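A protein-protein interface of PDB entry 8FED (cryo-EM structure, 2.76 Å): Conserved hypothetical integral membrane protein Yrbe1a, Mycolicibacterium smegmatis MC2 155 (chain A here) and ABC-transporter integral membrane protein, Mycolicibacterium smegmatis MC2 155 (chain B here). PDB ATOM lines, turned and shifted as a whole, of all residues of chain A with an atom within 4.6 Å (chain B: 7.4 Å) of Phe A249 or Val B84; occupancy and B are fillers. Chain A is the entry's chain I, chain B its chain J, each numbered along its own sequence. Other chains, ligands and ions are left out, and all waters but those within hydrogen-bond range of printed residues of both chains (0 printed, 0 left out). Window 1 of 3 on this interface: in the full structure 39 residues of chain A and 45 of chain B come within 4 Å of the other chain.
The backbone carbonyl oxygen (O) of Phe B83 sits at hydrogen-bond distance from the side-chain hydroxyl (OG) of Ser B87 (3.0 Å).
Among the printed residues, pairs that only touch across the chains: Val A245 with Val B84, Val A246 with Phe B83, Phe A249 with Val B84, Phe A249 with Ser B87, Asn A252 with Leu B91, Val A253 with Ser B87 and Val A253 with Leu B91.
Of the printed residues of chain A, Val B84 touches Val A245 (3.99 Å) and Phe A249 (3.7 Å).
Printed residues of chain A within 4 Å of Leu B91: Asn A252 and Val A253.
Of the printed residues of chain A, Ser B87 touches Phe A249 (3.9 Å) and Val A253 (3.7 Å).
Of the printed residues of chain B, Val A246 touches Phe B83.
Of the printed residues of chain B, Val A253 touches Ser B87 (3.7 Å) and Leu B91 (3.6 Å).
Printed residues of chain A within 4 Å of Phe B83: Val A246.
Val A251 touches none of the printed residues of chain B.
The nearest residue of chain B that does not touch Phe A249 is Val B125 (4.5 Å).
Of the 21 printed residues of chain B, 4 touch a printed residue of chain A.
Hydrophobic or aromatic side chains of chain B that line the printed part of chain A: Phe B83, Val B84 and Leu B91.
Hydrophobic or aromatic side chains of chain A that line the printed part of chain B: Val A245, Val A246, Phe A249 and Val A253.
Along chain A the printed residues that touch a printed residue of chain B span positions 245 to 253.
Among the printed residues, 7 pairs touch across the chains.
Among the printed residues, no Asp or Glu carboxylate lies within 4 Å of a Lys or Arg side-chain nitrogen of the other chain.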
ATOM      1  N   LEU A 105      11.056 -15.126   0.359  1.00  0.00           N
ATOM      2  CA  LEU A 105      10.890 -14.955  -1.083  1.00  0.00           C
ATOM      3  C   LEU A 105      11.748 -13.814  -1.618  1.00  0.00           C
ATOM      4  O   LEU A 105      12.344 -13.934  -2.695  1.00  0.00           O
ATOM      5  CB  LEU A 105       9.423 -14.722  -1.427  1.00  0.00           C
ATOM      6  CG  LEU A 105       8.606 -15.989  -1.664  1.00  0.00           C
ATOM      7  CD1 LEU A 105       7.201 -15.626  -2.091  1.00  0.00           C
ATOM      8  CD2 LEU A 105       9.282 -16.856  -2.712  1.00  0.00           C
ATOM      9  N   VAL A 245      15.727 -20.262  -9.414  1.00  0.00           N
ATOM     10  CA  VAL A 245      14.341 -19.847  -9.198  1.00  0.00           C
ATOM     11  C   VAL A 245      13.440 -21.065  -9.026  1.00  0.00           C
ATOM     12  O   VAL A 245      12.650 -21.145  -8.075  1.00  0.00           O
ATOM     13  CB  VAL A 245      13.863 -18.944 -10.348  1.00  0.00           C
ATOM     14  CG1 VAL A 245      12.359 -18.764 -10.292  1.00  0.00           C
ATOM     15  CG2 VAL A 245      14.551 -17.593 -10.275  1.00  0.00           C
ATOM     16  N   VAL A 246      13.574 -22.051  -9.917  1.00  0.00           N
ATOM     17  CA  VAL A 246      12.695 -23.219  -9.870  1.00  0.00           C
ATOM     18  C   VAL A 246      12.919 -24.014  -8.585  1.00  0.00           C
ATOM     19  O   VAL A 246      11.963 -24.367  -7.875  1.00  0.00           O
ATOM     20  CB  VAL A 246      12.901 -24.093 -11.120  1.00  0.00           C
ATOM     21  CG1 VAL A 246      12.135 -25.395 -10.990  1.00  0.00           C
ATOM     22  CG2 VAL A 246      12.459 -23.343 -12.363  1.00  0.00           C
ATOM     23  N   ALA A 247      14.184 -24.306  -8.266  1.00  0.00           N
ATOM     24  CA  ALA A 247      14.488 -25.114  -7.091  1.00  0.00           C
ATOM     25  C   ALA A 247      14.073 -24.410  -5.809  1.00  0.00           C
ATOM     26  O   ALA A 247      13.519 -25.042  -4.900  1.00  0.00           O
ATOM     27  CB  ALA A 247      15.978 -25.450  -7.059  1.00  0.00           C
ATOM     28  N   LEU A 248      14.322 -23.100  -5.712  1.00  0.00           N
ATOM     29  CA  LEU A 248      13.957 -22.380  -4.501  1.00  0.00           C
ATOM     30  C   LEU A 248      12.450 -22.265  -4.349  1.00  0.00           C
ATOM     31  O   LEU A 248      11.947 -22.324  -3.225  1.00  0.00           O
ATOM     32  CB  LEU A 248      14.618 -21.002  -4.473  1.00  0.00           C
ATOM     33  CG  LEU A 248      16.149 -21.013  -4.371  1.00  0.00           C
ATOM     34  CD1 LEU A 248      16.706 -19.629  -4.082  1.00  0.00           C
ATOM     35  CD2 LEU A 248      16.637 -22.025  -3.349  1.00  0.00           C
ATOM     36  N   PHE A 249      11.704 -22.124  -5.450  1.00  0.00           N
ATOM     37  CA  PHE A 249      10.249 -22.122  -5.327  1.00  0.00           C
ATOM     38  C   PHE A 249       9.723 -23.477  -4.865  1.00  0.00           C
ATOM     39  O   PHE A 249       8.819 -23.540  -4.021  1.00  0.00           O
ATOM     40  CB  PHE A 249       9.605 -21.706  -6.647  1.00  0.00           C
ATOM     41  CG  PHE A 249       9.276 -20.244  -6.720  1.00  0.00           C
ATOM     42  CD1 PHE A 249      10.210 -19.332  -7.177  1.00  0.00           C
ATOM     43  CD2 PHE A 249       8.037 -19.781  -6.322  1.00  0.00           C
ATOM     44  CE1 PHE A 249       9.912 -17.986  -7.239  1.00  0.00           C
ATOM     45  CE2 PHE A 249       7.733 -18.436  -6.382  1.00  0.00           C
ATOM     46  CZ  PHE A 249       8.671 -17.539  -6.842  1.00  0.00           C
ATOM     47  N   ALA A 250      10.274 -24.573  -5.396  1.00  0.00           N
ATOM     48  CA  ALA A 250       9.840 -25.896  -4.943  1.00  0.00           C
ATOM     49  C   ALA A 250      10.156 -26.111  -3.463  1.00  0.00           C
ATOM     50  O   ALA A 250       9.311 -26.604  -2.697  1.00  0.00           O
ATOM     51  CB  ALA A 250      10.494 -26.982  -5.794  1.00  0.00           C
ATOM     52  N   VAL A 251      11.369 -25.739  -3.042  1.00  0.00           N
ATOM     53  CA  VAL A 251      11.755 -25.877  -1.641  1.00  0.00           C
ATOM     54  C   VAL A 251      10.878 -24.995  -0.760  1.00  0.00           C
ATOM     55  O   VAL A 251      10.509 -25.379   0.355  1.00  0.00           O
ATOM     56  CB  VAL A 251      13.253 -25.561  -1.467  1.00  0.00           C
ATOM     57  CG1 VAL A 251      13.629 -25.494   0.002  1.00  0.00           C
ATOM     58  CG2 VAL A 251      14.093 -26.614  -2.166  1.00  0.00           C
ATOM     59  N   ASN A 252      10.524 -23.804  -1.249  1.00  0.00           N
ATOM     60  CA  ASN A 252       9.647 -22.918  -0.494  1.00  0.00           C
ATOM     61  C   ASN A 252       8.268 -23.535  -0.313  1.00  0.00           C
ATOM     62  O   ASN A 252       7.677 -23.426   0.764  1.00  0.00           O
ATOM     63  CB  ASN A 252       9.540 -21.564  -1.193  1.00  0.00           C
ATOM     64  CG  ASN A 252       8.738 -20.558  -0.396  1.00  0.00           C
ATOM     65  OD1 ASN A 252       8.576 -20.695   0.814  1.00  0.00           O
ATOM     66  ND2 ASN A 252       8.233 -19.538  -1.073  1.00  0.00           N
ATOM     67  N   VAL A 253       7.741 -24.185  -1.352  1.00  0.00           N
ATOM     68  CA  VAL A 253       6.445 -24.854  -1.225  1.00  0.00           C
ATOM     69  C   VAL A 253       6.513 -25.953  -0.168  1.00  0.00           C
ATOM     70  O   VAL A 253       5.642 -26.054   0.712  1.00  0.00           O
ATOM     71  CB  VAL A 253       5.986 -25.409  -2.586  1.00  0.00           C
ATOM     72  CG1 VAL A 253       4.758 -26.286  -2.416  1.00  0.00           C
ATOM     73  CG2 VAL A 253       5.688 -24.274  -3.544  1.00  0.00           C
ATOM     74  N   VAL B  78       7.492 -20.879 -21.279  1.00  0.00           N
ATOM     75  CA  VAL B  78       6.168 -21.350 -20.878  1.00  0.00           C
ATOM     76  C   VAL B  78       6.268 -22.278 -19.674  1.00  0.00           C
ATOM     77  O   VAL B  78       5.521 -22.140 -18.700  1.00  0.00           O
ATOM     78  CB  VAL B  78       5.460 -22.035 -22.061  1.00  0.00           C
ATOM     79  CG1 VAL B  78       4.170 -22.692 -21.602  1.00  0.00           C
ATOM     80  CG2 VAL B  78       5.172 -21.029 -23.158  1.00  0.00           C
ATOM     81  N   ALA B  79       7.204 -23.230 -19.718  1.00  0.00           N
ATOM     82  CA  ALA B  79       7.329 -24.198 -18.633  1.00  0.00           C
ATOM     83  C   ALA B  79       7.753 -23.532 -17.329  1.00  0.00           C
ATOM     84  O   ALA B  79       7.208 -23.843 -16.263  1.00  0.00           O
ATOM     85  CB  ALA B  79       8.319 -25.293 -19.019  1.00  0.00           C
ATOM     86  N   ILE B  80       8.724 -22.619 -17.391  1.00  0.00           N
ATOM     87  CA  ILE B  80       9.198 -21.951 -16.182  1.00  0.00           C
ATOM     88  C   ILE B  80       8.096 -21.087 -15.581  1.00  0.00           C
ATOM     89  O   ILE B  80       7.856 -21.114 -14.366  1.00  0.00           O
ATOM     90  CB  ILE B  80      10.461 -21.126 -16.484  1.00  0.00           C
ATOM     91  CG1 ILE B  80      11.516 -21.990 -17.179  1.00  0.00           C
ATOM     92  CG2 ILE B  80      11.024 -20.525 -15.207  1.00  0.00           C
ATOM     93  CD1 ILE B  80      11.856 -23.264 -16.437  1.00  0.00           C
ATOM     94  N   ILE B  81       7.407 -20.313 -16.426  1.00  0.00           N
ATOM     95  CA  ILE B  81       6.301 -19.483 -15.954  1.00  0.00           C
ATOM     96  C   ILE B  81       5.227 -20.352 -15.314  1.00  0.00           C
ATOM     97  O   ILE B  81       4.719 -20.038 -14.231  1.00  0.00           O
ATOM     98  CB  ILE B  81       5.730 -18.639 -17.109  1.00  0.00           C
ATOM     99  CG1 ILE B  81       6.734 -17.573 -17.559  1.00  0.00           C
ATOM    100  CG2 ILE B  81       4.400 -18.011 -16.714  1.00  0.00           C
ATOM    101  CD1 ILE B  81       6.657 -16.280 -16.786  1.00  0.00           C
ATOM    102  N   GLY B  82       4.883 -21.465 -15.964  1.00  0.00           N
ATOM    103  CA  GLY B  82       3.850 -22.332 -15.428  1.00  0.00           C
ATOM    104  C   GLY B  82       4.223 -22.926 -14.087  1.00  0.00           C
ATOM    105  O   GLY B  82       3.416 -22.935 -13.157  1.00  0.00           O
ATOM    106  N   PHE B  83       5.457 -23.422 -13.965  1.00  0.00           N
ATOM    107  CA  PHE B  83       5.886 -24.015 -12.702  1.00  0.00           C
ATOM    108  C   PHE B  83       5.896 -22.984 -11.580  1.00  0.00           C
ATOM    109  O   PHE B  83       5.415 -23.258 -10.471  1.00  0.00           O
ATOM    110  CB  PHE B  83       7.268 -24.648 -12.860  1.00  0.00           C
ATOM    111  CG  PHE B  83       7.692 -25.477 -11.682  1.00  0.00           C
ATOM    112  CD1 PHE B  83       8.422 -24.917 -10.646  1.00  0.00           C
ATOM    113  CD2 PHE B  83       7.358 -26.818 -11.610  1.00  0.00           C
ATOM    114  CE1 PHE B  83       8.809 -25.679  -9.562  1.00  0.00           C
ATOM    115  CE2 PHE B  83       7.745 -27.585 -10.528  1.00  0.00           C
ATOM    116  CZ  PHE B  83       8.471 -27.014  -9.504  1.00  0.00           C
ATOM    117  N   VAL B  84       6.426 -21.788 -11.848  1.00  0.00           N
ATOM    118  CA  VAL B  84       6.513 -20.779 -10.797  1.00  0.00           C
ATOM    119  C   VAL B  84       5.120 -20.313 -10.382  1.00  0.00           C
ATOM    120  O   VAL B  84       4.848 -20.110  -9.190  1.00  0.00           O
ATOM    121  CB  VAL B  84       7.411 -19.612 -11.251  1.00  0.00           C
ATOM    122  CG1 VAL B  84       7.468 -18.543 -10.191  1.00  0.00           C
ATOM    123  CG2 VAL B  84       8.814 -20.116 -11.522  1.00  0.00           C
ATOM    124  N   THR B  85       4.206 -20.156 -11.345  1.00  0.00           N
ATOM    125  CA  THR B  85       2.851 -19.729 -11.007  1.00  0.00           C
ATOM    126  C   THR B  85       2.089 -20.816 -10.258  1.00  0.00           C
ATOM    127  O   THR B  85       1.309 -20.512  -9.347  1.00  0.00           O
ATOM    128  CB  THR B  85       2.100 -19.309 -12.266  1.00  0.00           C
ATOM    129  OG1 THR B  85       2.232 -20.326 -13.266  1.00  0.00           O
ATOM    130  CG2 THR B  85       2.660 -18.002 -12.790  1.00  0.00           C
ATOM    131  N   LEU B  86       2.290 -22.086 -10.627  1.00  0.00           N
ATOM    132  CA  LEU B  86       1.691 -23.175  -9.864  1.00  0.00           C
ATOM    133  C   LEU B  86       2.194 -23.170  -8.428  1.00  0.00           C
ATOM    134  O   LEU B  86       1.412 -23.358  -7.486  1.00  0.00           O
ATOM    135  CB  LEU B  86       1.994 -24.522 -10.524  1.00  0.00           C
ATOM    136  CG  LEU B  86       1.309 -24.901 -11.840  1.00  0.00           C
ATOM    137  CD1 LEU B  86       1.865 -26.214 -12.357  1.00  0.00           C
ATOM    138  CD2 LEU B  86      -0.195 -24.992 -11.682  1.00  0.00           C
ATOM    139  N   SER B  87       3.498 -22.949  -8.241  1.00  0.00           N
ATOM    140  CA  SER B  87       4.053 -22.882  -6.893  1.00  0.00           C
ATOM    141  C   SER B  87       3.446 -21.728  -6.101  1.00  0.00           C
ATOM    142  O   SER B  87       3.083 -21.896  -4.931  1.00  0.00           O
ATOM    143  CB  SER B  87       5.573 -22.746  -6.959  1.00  0.00           C
ATOM    144  OG  SER B  87       6.150 -23.850  -7.632  1.00  0.00           O
ATOM    145  N   ALA B  88       3.323 -20.553  -6.723  1.00  0.00           N
ATOM    146  CA  ALA B  88       2.757 -19.398  -6.029  1.00  0.00           C
ATOM    147  C   ALA B  88       1.299 -19.633  -5.644  1.00  0.00           C
ATOM    148  O   ALA B  88       0.877 -19.290  -4.530  1.00  0.00           O
ATOM    149  CB  ALA B  88       2.887 -18.150  -6.898  1.00  0.00           C
ATOM    150  N   GLY B  89       0.511 -20.211  -6.555  1.00  0.00           N
ATOM    151  CA  GLY B  89      -0.874 -20.513  -6.236  1.00  0.00           C
ATOM    152  C   GLY B  89      -1.004 -21.530  -5.119  1.00  0.00           C
ATOM    153  O   GLY B  89      -1.866 -21.402  -4.242  1.00  0.00           O
ATOM    154  N   SER B  90      -0.151 -22.559  -5.136  1.00  0.00           N
ATOM    155  CA  SER B  90      -0.155 -23.537  -4.055  1.00  0.00           C
ATOM    156  C   SER B  90       0.191 -22.881  -2.725  1.00  0.00           C
ATOM    157  O   SER B  90      -0.415 -23.199  -1.696  1.00  0.00           O
ATOM    158  CB  SER B  90       0.822 -24.669  -4.365  1.00  0.00           C
ATOM    159  OG  SER B  90       0.427 -25.382  -5.522  1.00  0.00           O
ATOM    160  N   LEU B  91       1.162 -21.964  -2.728  1.00  0.00           N
ATOM    161  CA  LEU B  91       1.516 -21.253  -1.502  1.00  0.00           C
ATOM    162  C   LEU B  91       0.332 -20.457  -0.973  1.00  0.00           C
ATOM    163  O   LEU B  91       0.033 -20.491   0.231  1.00  0.00           O
ATOM    164  CB  LEU B  91       2.708 -20.331  -1.749  1.00  0.00           C
ATOM    165  CG  LEU B  91       4.045 -21.012  -2.014  1.00  0.00           C
ATOM    166  CD1 LEU B  91       5.129 -19.985  -2.261  1.00  0.00           C
ATOM    167  CD2 LEU B  91       4.395 -21.888  -0.842  1.00  0.00           C
ATOM    168  N   VAL B 121       0.282 -11.357  -5.906  1.00  0.00           N
ATOM    169  CA  VAL B 121       1.131 -12.533  -6.083  1.00  0.00           C
ATOM    170  C   VAL B 121       1.393 -12.813  -7.556  1.00  0.00           C
ATOM    171  O   VAL B 121       2.548 -12.827  -7.996  1.00  0.00           O
ATOM    172  CB  VAL B 121       0.515 -13.752  -5.378  1.00  0.00           C
ATOM    173  CG1 VAL B 121       1.244 -15.019  -5.788  1.00  0.00           C
ATOM    174  CG2 VAL B 121       0.576 -13.565  -3.874  1.00  0.00           C
ATOM    175  N   VAL B 125       4.982 -12.293  -9.439  1.00  0.00           N
ATOM    176  CA  VAL B 125       5.640 -13.578  -9.663  1.00  0.00           C
ATOM    177  C   VAL B 125       5.857 -13.825 -11.154  1.00  0.00           C
ATOM    178  O   VAL B 125       6.947 -14.236 -11.581  1.00  0.00           O
ATOM    179  CB  VAL B 125       4.818 -14.704  -9.006  1.00  0.00           C
ATOM    180  CG1 VAL B 125       5.020 -16.018  -9.721  1.00  0.00           C
ATOM    181  CG2 VAL B 125       5.189 -14.834  -7.538  1.00  0.00           C
ATOM    182  N   THR B 126       4.829 -13.572 -11.969  1.00  0.00           N
ATOM    183  CA  THR B 126       4.974 -13.702 -13.413  1.00  0.00           C
ATOM    184  C   THR B 126       6.003 -12.717 -13.942  1.00  0.00           C
ATOM    185  O   THR B 126       6.775 -13.045 -14.848  1.00  0.00           O
ATOM    186  CB  THR B 126       3.623 -13.489 -14.097  1.00  0.00           C
ATOM    187  OG1 THR B 126       2.664 -14.403 -13.552  1.00  0.00           O
ATOM    188  CG2 THR B 126       3.733 -13.724 -15.595  1.00  0.00           C
ATOM    189  N   GLN B 128       8.700 -11.576 -12.318  1.00  0.00           N
ATOM    190  CA  GLN B 128      10.043 -12.052 -11.988  1.00  0.00           C
ATOM    191  C   GLN B 128      10.441 -13.237 -12.860  1.00  0.00           C
ATOM    192  O   GLN B 128      11.580 -13.307 -13.335  1.00  0.00           O
ATOM    193  CB  GLN B 128      10.143 -12.427 -10.507  1.00  0.00           C
ATOM    194  CG  GLN B 128       9.627 -11.393  -9.497  1.00  0.00           C
ATOM    195  CD  GLN B 128      10.405 -10.084  -9.463  1.00  0.00           C
ATOM    196  OE1 GLN B 128      10.520  -9.382 -10.464  1.00  0.00           O
ATOM    197  NE2 GLN B 128      10.923  -9.742  -8.292  1.00  0.00           N
ATOM    198  N   ALA B 129       9.521 -14.181 -13.084  1.00  0.00           N
ATOM    199  CA  ALA B 129       9.850 -15.340 -13.912  1.00  0.00           C
ATOM    200  C   ALA B 129      10.089 -14.943 -15.366  1.00  0.00           C
ATOM    201  O   ALA B 129      11.034 -15.432 -16.004  1.00  0.00           O
ATOM    202  CB  ALA B 129       8.743 -16.387 -13.814  1.00  0.00           C
ATOM    203  N   SER B 188      -2.256 -20.283 -12.041  1.00  0.00           N
ATOM    204  CA  SER B 188      -2.340 -19.878 -10.641  1.00  0.00           C
ATOM    205  C   SER B 188      -3.712 -20.201 -10.060  1.00  0.00           C
ATOM    206  O   SER B 188      -3.818 -20.777  -8.968  1.00  0.00           O
ATOM    207  CB  SER B 188      -2.034 -18.386 -10.516  1.00  0.00           C
ATOM    208  OG  SER B 188      -2.073 -17.971  -9.165  1.00  0.00           O
ATOM    209  N   SER B 191      -4.052 -24.049  -9.736  1.00  0.00           N
ATOM    210  CA  SER B 191      -3.287 -24.588  -8.618  1.00  0.00           C
ATOM    211  C   SER B 191      -3.961 -24.274  -7.290  1.00  0.00           C
ATOM    212  O   SER B 191      -4.076 -25.148  -6.421  1.00  0.00           O
ATOM    213  CB  SER B 191      -1.866 -24.029  -8.639  1.00  0.00           C
ATOM    214  OG  SER B 191      -1.875 -22.618  -8.540  1.00  0.00           O
